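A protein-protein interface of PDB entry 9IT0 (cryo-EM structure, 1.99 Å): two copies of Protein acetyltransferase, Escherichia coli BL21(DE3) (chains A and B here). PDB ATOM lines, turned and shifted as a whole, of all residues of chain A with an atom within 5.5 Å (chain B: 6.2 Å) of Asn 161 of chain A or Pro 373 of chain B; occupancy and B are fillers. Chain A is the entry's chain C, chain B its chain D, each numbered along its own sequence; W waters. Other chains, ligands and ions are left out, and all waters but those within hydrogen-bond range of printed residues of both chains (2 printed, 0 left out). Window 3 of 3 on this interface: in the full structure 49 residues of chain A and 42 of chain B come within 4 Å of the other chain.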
ATOM      1  N   LEU A 127     -34.176 -20.240   1.615  1.00  0.00           N
ATOM      2  CA  LEU A 127     -32.980 -21.030   1.344  1.00  0.00           C
ATOM      3  C   LEU A 127     -33.112 -22.467   1.835  1.00  0.00           C
ATOM      4  O   LEU A 127     -32.448 -23.354   1.290  1.00  0.00           O
ATOM      5  CB  LEU A 127     -31.754 -20.369   1.985  1.00  0.00           C
ATOM      6  CG  LEU A 127     -30.405 -21.072   1.789  1.00  0.00           C
ATOM      7  CD1 LEU A 127     -30.037 -21.158   0.311  1.00  0.00           C
ATOM      8  CD2 LEU A 127     -29.308 -20.364   2.571  1.00  0.00           C
ATOM      9  N   SER A 141     -27.894 -24.532  -0.010  1.00  0.00           N
ATOM     10  CA  SER A 141     -26.671 -23.822   0.345  1.00  0.00           C
ATOM     11  C   SER A 141     -25.439 -24.641  -0.043  1.00  0.00           C
ATOM     12  O   SER A 141     -25.446 -25.867   0.087  1.00  0.00           O
ATOM     13  CB  SER A 141     -26.638 -23.530   1.843  1.00  0.00           C
ATOM     14  OG  SER A 141     -25.828 -24.458   2.532  1.00  0.00           O
ATOM     15  N   PRO A 142     -24.368 -24.011  -0.523  1.00  0.00           N
ATOM     16  CA  PRO A 142     -23.139 -24.753  -0.849  1.00  0.00           C
ATOM     17  C   PRO A 142     -22.141 -24.910   0.291  1.00  0.00           C
ATOM     18  O   PRO A 142     -21.015 -25.342   0.028  1.00  0.00           O
ATOM     19  CB  PRO A 142     -22.529 -23.896  -1.966  1.00  0.00           C
ATOM     20  CG  PRO A 142     -22.973 -22.504  -1.662  1.00  0.00           C
ATOM     21  CD  PRO A 142     -24.288 -22.598  -0.939  1.00  0.00           C
ATOM     22  N   VAL A 143     -22.498 -24.596   1.528  1.00  0.00           N
ATOM     23  CA  VAL A 143     -21.571 -24.615   2.661  1.00  0.00           C
ATOM     24  C   VAL A 143     -21.976 -25.751   3.596  1.00  0.00           C
ATOM     25  O   VAL A 143     -23.158 -25.865   3.933  1.00  0.00           O
ATOM     26  CB  VAL A 143     -21.560 -23.269   3.417  1.00  0.00           C
ATOM     27  CG1 VAL A 143     -20.405 -23.216   4.411  1.00  0.00           C
ATOM     28  CG2 VAL A 143     -21.463 -22.089   2.443  1.00  0.00           C
ATOM     29  N   SER A 156     -32.389 -13.586   5.609  1.00  0.00           N
ATOM     30  CA  SER A 156     -31.556 -13.248   4.456  1.00  0.00           C
ATOM     31  C   SER A 156     -30.628 -14.408   4.113  1.00  0.00           C
ATOM     32  O   SER A 156     -29.890 -14.894   4.975  1.00  0.00           O
ATOM     33  CB  SER A 156     -30.730 -11.983   4.726  1.00  0.00           C
ATOM     34  OG  SER A 156     -29.667 -11.859   3.799  1.00  0.00           O
ATOM     35  N   ALA A 157     -30.656 -14.833   2.844  1.00  0.00           N
ATOM     36  CA  ALA A 157     -29.838 -15.966   2.410  1.00  0.00           C
ATOM     37  C   ALA A 157     -28.345 -15.645   2.445  1.00  0.00           C
ATOM     38  O   ALA A 157     -27.532 -16.489   2.852  1.00  0.00           O
ATOM     39  CB  ALA A 157     -30.258 -16.399   1.005  1.00  0.00           C
ATOM     40  N   ALA A 158     -27.959 -14.444   2.003  1.00  0.00           N
ATOM     41  CA  ALA A 158     -26.541 -14.097   1.956  1.00  0.00           C
ATOM     42  C   ALA A 158     -25.920 -14.108   3.349  1.00  0.00           C
ATOM     43  O   ALA A 158     -24.808 -14.616   3.536  1.00  0.00           O
ATOM     44  CB  ALA A 158     -26.353 -12.732   1.294  1.00  0.00           C
ATOM     45  N   VAL A 159     -26.628 -13.557   4.338  1.00  0.00           N
ATOM     46  CA  VAL A 159     -26.122 -13.571   5.707  1.00  0.00           C
ATOM     47  C   VAL A 159     -25.979 -15.005   6.202  1.00  0.00           C
ATOM     48  O   VAL A 159     -25.022 -15.343   6.908  1.00  0.00           O
ATOM     49  CB  VAL A 159     -27.041 -12.742   6.626  1.00  0.00           C
ATOM     50  CG1 VAL A 159     -26.629 -12.910   8.081  1.00  0.00           C
ATOM     51  CG2 VAL A 159     -27.007 -11.271   6.230  1.00  0.00           C
ATOM     52  N   SER A 160     -26.936 -15.867   5.847  1.00  0.00           N
ATOM     53  CA  SER A 160     -26.871 -17.270   6.248  1.00  0.00           C
ATOM     54  C   SER A 160     -25.613 -17.936   5.703  1.00  0.00           C
ATOM     55  O   SER A 160     -24.881 -18.611   6.442  1.00  0.00           O
ATOM     56  CB  SER A 160     -28.119 -18.009   5.758  1.00  0.00           C
ATOM     57  OG  SER A 160     -29.300 -17.479   6.329  1.00  0.00           O
ATOM     58  N   ASN A 161     -25.348 -17.764   4.404  1.00  0.00           N
ATOM     59  CA  ASN A 161     -24.148 -18.361   3.819  1.00  0.00           C
ATOM     60  C   ASN A 161     -22.884 -17.799   4.465  1.00  0.00           C
ATOM     61  O   ASN A 161     -21.935 -18.544   4.747  1.00  0.00           O
ATOM     62  CB  ASN A 161     -24.140 -18.183   2.298  1.00  0.00           C
ATOM     63  CG  ASN A 161     -25.172 -19.055   1.590  1.00  0.00           C
ATOM     64  OD1 ASN A 161     -25.336 -20.230   1.919  1.00  0.00           O
ATOM     65  ND2 ASN A 161     -25.854 -18.489   0.604  1.00  0.00           N
ATOM     66  N   THR A 162     -22.855 -16.486   4.714  1.00  0.00           N
ATOM     67  CA  THR A 162     -21.682 -15.880   5.340  1.00  0.00           C
ATOM     68  C   THR A 162     -21.426 -16.468   6.724  1.00  0.00           C
ATOM     69  O   THR A 162     -20.283 -16.800   7.068  1.00  0.00           O
ATOM     70  CB  THR A 162     -21.869 -14.365   5.432  1.00  0.00           C
ATOM     71  OG1 THR A 162     -22.077 -13.825   4.121  1.00  0.00           O
ATOM     72  CG2 THR A 162     -20.658 -13.701   6.071  1.00  0.00           C
ATOM     73  N   ILE A 163     -22.479 -16.611   7.529  1.00  0.00           N
ATOM     74  CA  ILE A 163     -22.305 -17.128   8.882  1.00  0.00           C
ATOM     75  C   ILE A 163     -21.868 -18.587   8.841  1.00  0.00           C
ATOM     76  O   ILE A 163     -21.029 -19.017   9.642  1.00  0.00           O
ATOM     77  CB  ILE A 163     -23.599 -16.941   9.698  1.00  0.00           C
ATOM     78  CG1 ILE A 163     -23.838 -15.454   9.995  1.00  0.00           C
ATOM     79  CG2 ILE A 163     -23.537 -17.740  10.993  1.00  0.00           C
ATOM     80  CD1 ILE A 163     -22.802 -14.803  10.889  1.00  0.00           C
ATOM     81  N   LEU A 164     -22.429 -19.375   7.916  1.00  0.00           N
ATOM     82  CA  LEU A 164     -21.995 -20.764   7.785  1.00  0.00           C
ATOM     83  C   LEU A 164     -20.513 -20.846   7.425  1.00  0.00           C
ATOM     84  O   LEU A 164     -19.780 -21.681   7.970  1.00  0.00           O
ATOM     85  CB  LEU A 164     -22.841 -21.495   6.738  1.00  0.00           C
ATOM     86  CG  LEU A 164     -24.281 -21.840   7.143  1.00  0.00           C
ATOM     87  CD1 LEU A 164     -25.124 -22.201   5.929  1.00  0.00           C
ATOM     88  CD2 LEU A 164     -24.314 -22.976   8.149  1.00  0.00           C
ATOM     89  N   ASP A 165     -20.051 -19.985   6.512  1.00  0.00           N
ATOM     90  CA  ASP A 165     -18.634 -20.000   6.150  1.00  0.00           C
ATOM     91  C   ASP A 165     -17.757 -19.613   7.337  1.00  0.00           C
ATOM     92  O   ASP A 165     -16.706 -20.229   7.577  1.00  0.00           O
ATOM     93  CB  ASP A 165     -18.387 -19.063   4.969  1.00  0.00           C
ATOM     94  CG  ASP A 165     -17.249 -19.528   4.084  1.00  0.00           C
ATOM     95  OD1 ASP A 165     -17.501 -20.329   3.160  1.00  0.00           O
ATOM     96  OD2 ASP A 165     -16.100 -19.097   4.314  1.00  0.00           O
ATOM     97  N   TRP A 166     -18.182 -18.604   8.102  1.00  0.00           N
ATOM     98  CA  TRP A 166     -17.425 -18.223   9.289  1.00  0.00           C
ATOM     99  C   TRP A 166     -17.330 -19.386  10.269  1.00  0.00           C
ATOM    100  O   TRP A 166     -16.254 -19.672  10.803  1.00  0.00           O
ATOM    101  CB  TRP A 166     -18.073 -17.011   9.958  1.00  0.00           C
ATOM    102  CG  TRP A 166     -17.257 -16.435  11.075  1.00  0.00           C
ATOM    103  CD1 TRP A 166     -16.387 -15.386  10.998  1.00  0.00           C
ATOM    104  CD2 TRP A 166     -17.229 -16.879  12.436  1.00  0.00           C
ATOM    105  NE1 TRP A 166     -15.823 -15.148  12.228  1.00  0.00           N
ATOM    106  CE2 TRP A 166     -16.323 -16.051  13.128  1.00  0.00           C
ATOM    107  CE3 TRP A 166     -17.884 -17.896  13.137  1.00  0.00           C
ATOM    108  CZ2 TRP A 166     -16.056 -16.208  14.486  1.00  0.00           C
ATOM    109  CZ3 TRP A 166     -17.618 -18.050  14.484  1.00  0.00           C
ATOM    110  CH2 TRP A 166     -16.712 -17.210  15.145  1.00  0.00           C
ATOM    111  N   ASN B 296     -24.076  -9.014  -5.092  1.00  0.00           N
ATOM    112  CA  ASN B 296     -24.898 -10.181  -5.416  1.00  0.00           C
ATOM    113  C   ASN B 296     -25.822 -10.537  -4.257  1.00  0.00           C
ATOM    114  O   ASN B 296     -26.065 -11.711  -3.968  1.00  0.00           O
ATOM    115  CB  ASN B 296     -24.030 -11.376  -5.817  1.00  0.00           C
ATOM    116  CG  ASN B 296     -23.250 -11.969  -4.654  1.00  0.00           C
ATOM    117  OD1 ASN B 296     -22.895 -11.272  -3.706  1.00  0.00           O
ATOM    118  ND2 ASN B 296     -22.975 -13.267  -4.732  1.00  0.00           N
ATOM    119  N   HIS B 371     -19.118  -9.450  -2.918  1.00  0.00           N
ATOM    120  CA  HIS B 371     -19.394 -10.817  -3.360  1.00  0.00           C
ATOM    121  C   HIS B 371     -19.651 -11.718  -2.157  1.00  0.00           C
ATOM    122  O   HIS B 371     -18.842 -11.759  -1.225  1.00  0.00           O
ATOM    123  CB  HIS B 371     -18.234 -11.390  -4.190  1.00  0.00           C
ATOM    124  CG  HIS B 371     -18.437 -12.814  -4.612  1.00  0.00           C
ATOM    125  ND1 HIS B 371     -18.089 -13.885  -3.817  1.00  0.00           N
ATOM    126  CD2 HIS B 371     -18.950 -13.342  -5.749  1.00  0.00           C
ATOM    127  CE1 HIS B 371     -18.382 -15.010  -4.445  1.00  0.00           C
ATOM    128  NE2 HIS B 371     -18.905 -14.708  -5.619  1.00  0.00           N
ATOM    129  N   SER B 372     -20.771 -12.456  -2.192  1.00  0.00           N
ATOM    130  CA  SER B 372     -21.119 -13.425  -1.160  1.00  0.00           C
ATOM    131  C   SER B 372     -21.077 -14.849  -1.713  1.00  0.00           C
ATOM    132  O   SER B 372     -21.266 -15.059  -2.915  1.00  0.00           O
ATOM    133  CB  SER B 372     -22.517 -13.152  -0.592  1.00  0.00           C
ATOM    134  OG  SER B 372     -22.447 -12.350   0.568  1.00  0.00           O
ATOM    135  N   PRO B 373     -20.852 -15.854  -0.864  1.00  0.00           N
ATOM    136  CA  PRO B 373     -20.706 -17.225  -1.372  1.00  0.00           C
ATOM    137  C   PRO B 373     -21.958 -17.688  -2.104  1.00  0.00           C
ATOM    138  O   PRO B 373     -23.083 -17.452  -1.659  1.00  0.00           O
ATOM    139  CB  PRO B 373     -20.450 -18.054  -0.105  1.00  0.00           C
ATOM    140  CG  PRO B 373     -20.089 -17.062   0.958  1.00  0.00           C
ATOM    141  CD  PRO B 373     -20.805 -15.806   0.607  1.00  0.00           C
ATOM    142  N   SER B 374     -21.750 -18.366  -3.231  1.00  0.00           N
ATOM    143  CA  SER B 374     -22.859 -18.814  -4.061  1.00  0.00           C
ATOM    144  C   SER B 374     -22.378 -19.916  -4.993  1.00  0.00           C
ATOM    145  O   SER B 374     -21.185 -20.032  -5.286  1.00  0.00           O
ATOM    146  CB  SER B 374     -23.458 -17.654  -4.866  1.00  0.00           C
ATOM    147  OG  SER B 374     -22.737 -17.436  -6.067  1.00  0.00           O
ATOM    148  N   ALA B 375     -23.332 -20.728  -5.454  1.00  0.00           N
ATOM    149  CA  ALA B 375     -23.021 -21.800  -6.391  1.00  0.00           C
ATOM    150  C   ALA B 375     -22.803 -21.285  -7.807  1.00  0.00           C
ATOM    151  O   ALA B 375     -21.966 -21.828  -8.537  1.00  0.00           O
ATOM    152  CB  ALA B 375     -24.140 -22.843  -6.385  1.00  0.00           C
ATOM    153  N   ALA B 377     -21.570 -18.364  -8.841  1.00  0.00           N
ATOM    154  CA  ALA B 377     -20.354 -17.564  -9.003  1.00  0.00           C
ATOM    155  C   ALA B 377     -19.327 -17.960  -7.950  1.00  0.00           C
ATOM    156  O   ALA B 377     -19.305 -17.399  -6.846  1.00  0.00           O
ATOM    157  CB  ALA B 377     -20.665 -16.071  -8.921  1.00  0.00           C
ATOM    158  N   CYS B 406     -16.921 -11.582   1.154  1.00  0.00           N
ATOM    159  CA  CYS B 406     -17.296 -12.133   2.446  1.00  0.00           C
ATOM    160  C   CYS B 406     -17.227 -13.655   2.428  1.00  0.00           C
ATOM    161  O   CYS B 406     -17.457 -14.300   1.401  1.00  0.00           O
ATOM    162  CB  CYS B 406     -18.705 -11.676   2.829  1.00  0.00           C
ATOM    163  SG  CYS B 406     -18.973  -9.891   2.690  1.00  0.00           S
ATOM    164  N   GLY B 407     -16.903 -14.226   3.585  1.00  0.00           N
ATOM    165  CA  GLY B 407     -16.733 -15.661   3.725  1.00  0.00           C
ATOM    166  C   GLY B 407     -15.286 -16.016   3.999  1.00  0.00           C
ATOM    167  O   GLY B 407     -14.468 -16.072   3.078  1.00  0.00           O
ATOM    168  N   SER B 410     -13.723 -19.635   2.380  1.00  0.00           N
ATOM    169  CA  SER B 410     -13.735 -19.869   0.941  1.00  0.00           C
ATOM    170  C   SER B 410     -13.056 -18.778   0.116  1.00  0.00           C
ATOM    171  O   SER B 410     -12.889 -18.966  -1.093  1.00  0.00           O
ATOM    172  CB  SER B 410     -15.182 -20.031   0.457  1.00  0.00           C
ATOM    173  OG  SER B 410     -15.830 -18.775   0.355  1.00  0.00           O
HETATM  174  O   HOH W   1     -24.658 -15.911  -0.640  1.00  0.00           O
HETATM  175  O   HOH W   2     -22.408 -11.116   3.112  1.00  0.00           O
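Ala 158 of chain A touches Ser 372 of chain B (CB to OG, 3.99 Å). Pro 373 of chain B touches Asn 161 of chain A. OG of Ser 372 of chain B touches OG1 of Thr 162 of chain A, at 3.9 Å. C of Gly 407 of chain B touches OD2 of Asp 165 of chain A (3.2 Å).
Water W1 lies within hydrogen-bond range of O of Pro 373 of chain B and ND2 of Asn 161 of chain A. Water W2 lies within hydrogen-bond range of the side-chain hydroxyl (OG) of Ser 372 of chain B (2.8 Å), the side-chain hydroxyl (OG1) of Thr 162 of chain A (2.9 Å) and the side-chain sulfur (SG) of Cys 406 of chain B (3.7 Å).
The side-chain amide nitrogen (ND2) of Asn 161 of chain A sits at hydrogen-bond distance from the backbone carbonyl oxygen (O) of Ala 157 of chain A (3.4 Å). The backbone carbonyl oxygen of Ala 158 of chain A sits at hydrogen-bond distance from the side-chain hydroxyl of Thr 162 of chain A (2.9 Å). The backbone NH of Ser 372 of chain B lies within hydrogen-bond range of the side-chain amide oxygen of Asn 296 of chain B.
N of Ser 410 of chain B is in hydrogen-bond range of OD2 of Asp 165 of chain A, at 3.1 Å.
Of the printed residues of chain B, Ala 158 of chain A touches Ser 372 (3.99 Å). Asn 296 of chain B touches none of the printed residues of chain A. Printed residues of chain A within 4 Å of Ser 372 of chain B: Ala 158 (3.99 Å) and Thr 162 (3.9 Å). Pro 373 of chain B touches just one residue of chain A: Asn 161. Of the printed residues of chain A, Gly 407 of chain B touches Asp 165. Printed residues of chain A within 4 Å of Ser 410 of chain B: Asp 165. The nearest residue of chain B that does not touch Asn 161 of chain A is Ser 374 of chain B (5.6 Å). The nearest printed residue of chain B that does not touch Asp 165 of chain A is Pro 373 of chain B (4.7 Å).
No position is printed for both chains.
Hydrophobic or aromatic side chains of chain A that line the printed part of chain B: Ala 158. Among the printed residues, no Asp or Glu carboxylate lies within 4 Å of a Lys or Arg side-chain nitrogen of the other chain.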
